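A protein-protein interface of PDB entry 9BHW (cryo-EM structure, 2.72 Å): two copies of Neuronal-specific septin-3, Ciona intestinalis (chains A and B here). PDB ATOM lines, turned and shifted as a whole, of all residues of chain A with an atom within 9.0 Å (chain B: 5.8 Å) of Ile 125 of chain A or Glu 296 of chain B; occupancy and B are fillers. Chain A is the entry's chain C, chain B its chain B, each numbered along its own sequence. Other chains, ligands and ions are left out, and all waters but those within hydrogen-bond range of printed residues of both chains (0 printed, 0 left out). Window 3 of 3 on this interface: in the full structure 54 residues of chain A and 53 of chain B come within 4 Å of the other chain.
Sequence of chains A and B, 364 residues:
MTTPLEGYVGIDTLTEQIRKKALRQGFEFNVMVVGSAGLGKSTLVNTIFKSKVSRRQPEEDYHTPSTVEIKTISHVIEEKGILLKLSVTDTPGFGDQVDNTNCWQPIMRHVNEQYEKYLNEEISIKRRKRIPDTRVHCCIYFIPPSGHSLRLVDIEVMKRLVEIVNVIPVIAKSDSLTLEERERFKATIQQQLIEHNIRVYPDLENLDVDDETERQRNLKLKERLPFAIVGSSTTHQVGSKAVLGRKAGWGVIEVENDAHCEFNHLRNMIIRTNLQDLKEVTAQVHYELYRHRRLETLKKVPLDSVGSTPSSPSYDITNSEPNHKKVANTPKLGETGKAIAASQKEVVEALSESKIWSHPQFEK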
ATOM      1  N   LEU A 119      12.886 -11.358  -1.615  1.00  0.00           N
ATOM      2  CA  LEU A 119      12.062 -10.156  -1.587  1.00  0.00           C
ATOM      3  C   LEU A 119      12.713  -9.009  -2.346  1.00  0.00           C
ATOM      4  O   LEU A 119      12.031  -8.269  -3.066  1.00  0.00           O
ATOM      5  CB  LEU A 119      11.777  -9.744  -0.148  1.00  0.00           C
ATOM      6  CG  LEU A 119      10.868  -8.527  -0.032  1.00  0.00           C
ATOM      7  CD1 LEU A 119       9.575  -8.795  -0.749  1.00  0.00           C
ATOM      8  CD2 LEU A 119      10.607  -8.196   1.417  1.00  0.00           C
ATOM      9  N   ASN A 120      14.024  -8.839  -2.196  1.00  0.00           N
ATOM     10  CA  ASN A 120      14.699  -7.722  -2.834  1.00  0.00           C
ATOM     11  C   ASN A 120      14.804  -7.923  -4.335  1.00  0.00           C
ATOM     12  O   ASN A 120      14.844  -6.943  -5.086  1.00  0.00           O
ATOM     13  CB  ASN A 120      16.080  -7.525  -2.213  1.00  0.00           C
ATOM     14  CG  ASN A 120      16.022  -6.825  -0.867  1.00  0.00           C
ATOM     15  OD1 ASN A 120      14.954  -6.428  -0.403  1.00  0.00           O
ATOM     16  ND2 ASN A 120      17.175  -6.674  -0.230  1.00  0.00           N
ATOM     17  N   GLU A 121      14.851  -9.173  -4.795  1.00  0.00           N
ATOM     18  CA  GLU A 121      14.784  -9.397  -6.232  1.00  0.00           C
ATOM     19  C   GLU A 121      13.367  -9.222  -6.763  1.00  0.00           C
ATOM     20  O   GLU A 121      13.188  -8.774  -7.900  1.00  0.00           O
ATOM     21  CB  GLU A 121      15.315 -10.786  -6.577  1.00  0.00           C
ATOM     22  CG  GLU A 121      15.329 -11.095  -8.059  1.00  0.00           C
ATOM     23  CD  GLU A 121      16.286 -10.214  -8.838  1.00  0.00           C
ATOM     24  OE1 GLU A 121      17.267  -9.720  -8.244  1.00  0.00           O
ATOM     25  OE2 GLU A 121      16.056 -10.016 -10.050  1.00  0.00           O
ATOM     26  N   GLU A 122      12.356  -9.556  -5.961  1.00  0.00           N
ATOM     27  CA  GLU A 122      10.973  -9.402  -6.400  1.00  0.00           C
ATOM     28  C   GLU A 122      10.578  -7.933  -6.514  1.00  0.00           C
ATOM     29  O   GLU A 122       9.989  -7.518  -7.518  1.00  0.00           O
ATOM     30  CB  GLU A 122      10.043 -10.137  -5.438  1.00  0.00           C
ATOM     31  CG  GLU A 122       8.584 -10.076  -5.815  1.00  0.00           C
ATOM     32  CD  GLU A 122       7.707 -10.829  -4.843  1.00  0.00           C
ATOM     33  OE1 GLU A 122       8.245 -11.386  -3.864  1.00  0.00           O
ATOM     34  OE2 GLU A 122       6.476 -10.864  -5.052  1.00  0.00           O
ATOM     35  N   ILE A 123      10.886  -7.129  -5.493  1.00  0.00           N
ATOM     36  CA  ILE A 123      10.513  -5.715  -5.524  1.00  0.00           C
ATOM     37  C   ILE A 123      11.323  -4.953  -6.570  1.00  0.00           C
ATOM     38  O   ILE A 123      10.882  -3.909  -7.067  1.00  0.00           O
ATOM     39  CB  ILE A 123      10.663  -5.090  -4.123  1.00  0.00           C
ATOM     40  CG1 ILE A 123       9.714  -5.751  -3.134  1.00  0.00           C
ATOM     41  CG2 ILE A 123      10.372  -3.602  -4.141  1.00  0.00           C
ATOM     42  CD1 ILE A 123       9.987  -5.365  -1.701  1.00  0.00           C
ATOM     43  N   SER A 124      12.495  -5.465  -6.943  1.00  0.00           N
ATOM     44  CA  SER A 124      13.362  -4.765  -7.880  1.00  0.00           C
ATOM     45  C   SER A 124      12.652  -4.509  -9.203  1.00  0.00           C
ATOM     46  O   SER A 124      11.958  -5.379  -9.734  1.00  0.00           O
ATOM     47  CB  SER A 124      14.633  -5.573  -8.124  1.00  0.00           C
ATOM     48  OG  SER A 124      15.423  -4.980  -9.136  1.00  0.00           O
ATOM     49  N   ILE A 125      12.829  -3.297  -9.732  1.00  0.00           N
ATOM     50  CA  ILE A 125      12.151  -2.917 -10.967  1.00  0.00           C
ATOM     51  C   ILE A 125      12.731  -3.676 -12.152  1.00  0.00           C
ATOM     52  O   ILE A 125      11.991  -4.162 -13.015  1.00  0.00           O
ATOM     53  CB  ILE A 125      12.220  -1.395 -11.169  1.00  0.00           C
ATOM     54  CG1 ILE A 125      11.428  -0.688 -10.074  1.00  0.00           C
ATOM     55  CG2 ILE A 125      11.660  -1.020 -12.516  1.00  0.00           C
ATOM     56  CD1 ILE A 125      11.852   0.730  -9.834  1.00  0.00           C
ATOM     57  N   LYS A 126      14.055  -3.796 -12.217  1.00  0.00           N
ATOM     58  CA  LYS A 126      14.699  -4.631 -13.231  1.00  0.00           C
ATOM     59  C   LYS A 126      14.778  -6.071 -12.715  1.00  0.00           C
ATOM     60  O   LYS A 126      15.822  -6.575 -12.298  1.00  0.00           O
ATOM     61  CB  LYS A 126      16.069  -4.074 -13.590  1.00  0.00           C
ATOM     62  CG  LYS A 126      16.727  -4.761 -14.770  1.00  0.00           C
ATOM     63  CD  LYS A 126      15.966  -4.516 -16.059  1.00  0.00           C
ATOM     64  CE  LYS A 126      16.232  -3.121 -16.600  1.00  0.00           C
ATOM     65  NZ  LYS A 126      15.638  -2.928 -17.951  1.00  0.00           N
ATOM     66  N   ARG A 127      13.625  -6.728 -12.752  1.00  0.00           N
ATOM     67  CA  ARG A 127      13.464  -8.062 -12.199  1.00  0.00           C
ATOM     68  C   ARG A 127      13.781  -9.118 -13.247  1.00  0.00           C
ATOM     69  O   ARG A 127      13.515  -8.940 -14.439  1.00  0.00           O
ATOM     70  CB  ARG A 127      12.033  -8.247 -11.700  1.00  0.00           C
ATOM     71  CG  ARG A 127      11.755  -9.570 -11.037  1.00  0.00           C
ATOM     72  CD  ARG A 127      10.302  -9.962 -11.205  1.00  0.00           C
ATOM     73  NE  ARG A 127       9.400  -9.110 -10.444  1.00  0.00           N
ATOM     74  CZ  ARG A 127       8.080  -9.212 -10.472  1.00  0.00           C
ATOM     75  NH1 ARG A 127       7.475 -10.119 -11.220  1.00  0.00           N
ATOM     76  NH2 ARG A 127       7.347  -8.388  -9.731  1.00  0.00           N
ATOM     77  N   ARG A 128      14.359 -10.227 -12.796  1.00  0.00           N
ATOM     78  CA  ARG A 128      14.624 -11.334 -13.699  1.00  0.00           C
ATOM     79  C   ARG A 128      13.373 -12.174 -13.914  1.00  0.00           C
ATOM     80  O   ARG A 128      12.459 -12.195 -13.085  1.00  0.00           O
ATOM     81  CB  ARG A 128      15.767 -12.206 -13.182  1.00  0.00           C
ATOM     82  CG  ARG A 128      17.106 -11.494 -13.183  1.00  0.00           C
ATOM     83  CD  ARG A 128      18.229 -12.364 -12.648  1.00  0.00           C
ATOM     84  NE  ARG A 128      18.097 -12.654 -11.227  1.00  0.00           N
ATOM     85  CZ  ARG A 128      18.875 -13.499 -10.567  1.00  0.00           C
ATOM     86  NH1 ARG A 128      19.828 -14.182 -11.180  1.00  0.00           N
ATOM     87  NH2 ARG A 128      18.699 -13.657  -9.259  1.00  0.00           N
ATOM     88  N   ARG B 291       5.289  -4.027 -16.386  1.00  0.00           N
ATOM     89  CA  ARG B 291       5.673  -3.763 -15.007  1.00  0.00           C
ATOM     90  C   ARG B 291       6.909  -2.884 -14.943  1.00  0.00           C
ATOM     91  O   ARG B 291       6.969  -1.939 -14.149  1.00  0.00           O
ATOM     92  CB  ARG B 291       5.906  -5.090 -14.287  1.00  0.00           C
ATOM     93  CG  ARG B 291       6.067  -4.982 -12.793  1.00  0.00           C
ATOM     94  CD  ARG B 291       7.449  -5.428 -12.378  1.00  0.00           C
ATOM     95  NE  ARG B 291       7.560  -5.566 -10.934  1.00  0.00           N
ATOM     96  CZ  ARG B 291       8.709  -5.601 -10.279  1.00  0.00           C
ATOM     97  NH1 ARG B 291       9.866  -5.513 -10.913  1.00  0.00           N
ATOM     98  NH2 ARG B 291       8.698  -5.726  -8.956  1.00  0.00           N
ATOM     99  N   HIS B 292       7.897  -3.168 -15.790  1.00  0.00           N
ATOM    100  CA  HIS B 292       9.098  -2.346 -15.842  1.00  0.00           C
ATOM    101  C   HIS B 292       8.763  -0.910 -16.218  1.00  0.00           C
ATOM    102  O   HIS B 292       9.205   0.036 -15.554  1.00  0.00           O
ATOM    103  CB  HIS B 292      10.089  -2.954 -16.832  1.00  0.00           C
ATOM    104  CG  HIS B 292      11.341  -2.157 -17.004  1.00  0.00           C
ATOM    105  ND1 HIS B 292      11.459  -1.147 -17.931  1.00  0.00           N
ATOM    106  CD2 HIS B 292      12.536  -2.233 -16.375  1.00  0.00           C
ATOM    107  CE1 HIS B 292      12.671  -0.629 -17.862  1.00  0.00           C
ATOM    108  NE2 HIS B 292      13.344  -1.270 -16.925  1.00  0.00           N
ATOM    109  N   ARG B 293       7.954  -0.728 -17.265  1.00  0.00           N
ATOM    110  CA  ARG B 293       7.622   0.620 -17.715  1.00  0.00           C
ATOM    111  C   ARG B 293       6.848   1.387 -16.653  1.00  0.00           C
ATOM    112  O   ARG B 293       7.117   2.567 -16.406  1.00  0.00           O
ATOM    113  CB  ARG B 293       6.822   0.565 -19.014  1.00  0.00           C
ATOM    114  CG  ARG B 293       7.656   0.351 -20.256  1.00  0.00           C
ATOM    115  CD  ARG B 293       6.872   0.723 -21.498  1.00  0.00           C
ATOM    116  NE  ARG B 293       5.782  -0.208 -21.760  1.00  0.00           N
ATOM    117  CZ  ARG B 293       4.507   0.036 -21.490  1.00  0.00           C
ATOM    118  NH1 ARG B 293       4.122   1.178 -20.944  1.00  0.00           N
ATOM    119  NH2 ARG B 293       3.595  -0.889 -21.773  1.00  0.00           N
ATOM    120  N   ARG B 294       5.875   0.739 -16.015  1.00  0.00           N
ATOM    121  CA  ARG B 294       5.066   1.453 -15.036  1.00  0.00           C
ATOM    122  C   ARG B 294       5.856   1.759 -13.772  1.00  0.00           C
ATOM    123  O   ARG B 294       5.700   2.835 -13.183  1.00  0.00           O
ATOM    124  CB  ARG B 294       3.801   0.668 -14.706  1.00  0.00           C
ATOM    125  CG  ARG B 294       2.911   1.434 -13.761  1.00  0.00           C
ATOM    126  CD  ARG B 294       1.603   0.749 -13.479  1.00  0.00           C
ATOM    127  NE  ARG B 294       0.842   1.506 -12.493  1.00  0.00           N
ATOM    128  CZ  ARG B 294       0.030   2.511 -12.783  1.00  0.00           C
ATOM    129  NH1 ARG B 294      -0.128   2.934 -14.026  1.00  0.00           N
ATOM    130  NH2 ARG B 294      -0.634   3.112 -11.800  1.00  0.00           N
ATOM    131  N   LEU B 295       6.718   0.842 -13.336  1.00  0.00           N
ATOM    132  CA  LEU B 295       7.478   1.102 -12.123  1.00  0.00           C
ATOM    133  C   LEU B 295       8.591   2.118 -12.357  1.00  0.00           C
ATOM    134  O   LEU B 295       8.956   2.858 -11.432  1.00  0.00           O
ATOM    135  CB  LEU B 295       8.036  -0.207 -11.572  1.00  0.00           C
ATOM    136  CG  LEU B 295       7.006  -1.097 -10.872  1.00  0.00           C
ATOM    137  CD1 LEU B 295       7.681  -2.276 -10.212  1.00  0.00           C
ATOM    138  CD2 LEU B 295       6.213  -0.313  -9.851  1.00  0.00           C
ATOM    139  N   GLU B 296       9.097   2.209 -13.588  1.00  0.00           N
ATOM    140  CA  GLU B 296      10.111   3.196 -13.934  1.00  0.00           C
ATOM    141  C   GLU B 296       9.501   4.593 -13.955  1.00  0.00           C
ATOM    142  O   GLU B 296      10.209   5.586 -14.146  1.00  0.00           O
ATOM    143  CB  GLU B 296      10.722   2.865 -15.295  1.00  0.00           C
ATOM    144  CG  GLU B 296      12.189   3.197 -15.442  1.00  0.00           C
ATOM    145  CD  GLU B 296      13.044   2.528 -14.393  1.00  0.00           C
ATOM    146  OE1 GLU B 296      12.957   1.290 -14.263  1.00  0.00           O
ATOM    147  OE2 GLU B 296      13.814   3.229 -13.706  1.00  0.00           O
ATOM    148  N   THR B 297       8.182   4.673 -13.782  1.00  0.00           N
ATOM    149  CA  THR B 297       7.468   5.939 -13.697  1.00  0.00           C
ATOM    150  C   THR B 297       6.997   6.142 -12.265  1.00  0.00           C
ATOM    151  O   THR B 297       6.906   7.271 -11.774  1.00  0.00           O
ATOM    152  CB  THR B 297       6.282   5.956 -14.667  1.00  0.00           C
ATOM    153  OG1 THR B 297       6.753   5.783 -16.008  1.00  0.00           O
ATOM    154  CG2 THR B 297       5.518   7.267 -14.576  1.00  0.00           C
ATOM    155  N   LEU B 298       6.707   5.033 -11.586  1.00  0.00           N
ATOM    156  CA  LEU B 298       6.302   5.044 -10.188  1.00  0.00           C
ATOM    157  C   LEU B 298       7.469   4.804  -9.238  1.00  0.00           C
ATOM    158  O   LEU B 298       7.269   4.237  -8.156  1.00  0.00           O
ATOM    159  CB  LEU B 298       5.211   3.999  -9.955  1.00  0.00           C
ATOM    160  CG  LEU B 298       3.886   4.208 -10.683  1.00  0.00           C
ATOM    161  CD1 LEU B 298       2.953   3.039 -10.418  1.00  0.00           C
ATOM    162  CD2 LEU B 298       3.242   5.520 -10.264  1.00  0.00           C
ATOM    163  N   LYS B 299       8.686   5.204  -9.620  1.00  0.00           N
ATOM    164  CA  LYS B 299       9.848   5.092  -8.742  1.00  0.00           C
ATOM    165  C   LYS B 299       9.596   5.716  -7.374  1.00  0.00           C
ATOM    166  O   LYS B 299      10.175   5.283  -6.373  1.00  0.00           O
ATOM    167  CB  LYS B 299      11.074   5.778  -9.349  1.00  0.00           C
ATOM    168  CG  LYS B 299      11.451   5.376 -10.752  1.00  0.00           C
ATOM    169  CD  LYS B 299      12.658   6.191 -11.191  1.00  0.00           C
ATOM    170  CE  LYS B 299      12.943   6.043 -12.672  1.00  0.00           C
ATOM    171  NZ  LYS B 299      14.159   6.796 -13.082  1.00  0.00           N
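The side-chain carboxylate of Glu 296 of chain B lies within salt-bridge range of the side-chain amino group of Lys 299 of chain B (3.6 Å).
The guanidinium group of Arg 127 of chain A is in hydrogen-bond range of the backbone carbonyl oxygen of Glu 122 of chain A.
Ile 125 of chain A touches His 292 of chain B.
Leu 295 of chain B touches Ile 125 of chain A.
Glu 296 of chain B touches Ile 125 of chain A (OE1 to CG2, 3.2 Å).
Leu 119 of chain A touches none of the printed residues of chain B.
Of the printed residues of chain B, Glu 122 of chain A touches Arg 291.
Of the printed residues of chain A, Leu 295 of chain B touches Ile 125 (3.7 Å).
Glu 296 of chain B touches just one residue of chain A: Ile 125.
Lys 299 of chain B touches none of the printed residues of chain A.
The nearest residue of chain B that does not touch Ile 125 of chain A is Lys 299 of chain B (4.8 Å).
The nearest printed residue of chain B that does not touch Ser 124 of chain A is Leu 295 of chain B (5.3 Å).
Of the 10 printed residues of chain A, 6 touch a printed residue of chain B.
Hydrophobic or aromatic side chains of chain A that line the printed part of chain B: Ile 125.
The guanidinium group (NH2) of Arg 291 of chain B sits at hydrogen-bond distance from the backbone carbonyl oxygen (O) of Glu 122 of chain A, at 2.6 Å.
The guanidinium group (NH2) of Arg 291 of chain B is in hydrogen-bond range of the backbone carbonyl oxygen (O) of Ile 123 of chain A, at 3.4 Å.
NH1 of Arg 291 of chain B lies within hydrogen-bond range of O of Ser 124 of chain A.
NH1 of Arg 291 of chain B is in hydrogen-bond range of O of Ile 125 of chain A.
A ring nitrogen (NE2) of His 292 of chain B lies within hydrogen-bond range of the side-chain amino group of Lys 126 of chain A, at 3.0 Å.
NH2 of Arg 127 of chain A sits close to NE of Arg 291 of chain B, at 3.1 Å.
No position is printed for both chains.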
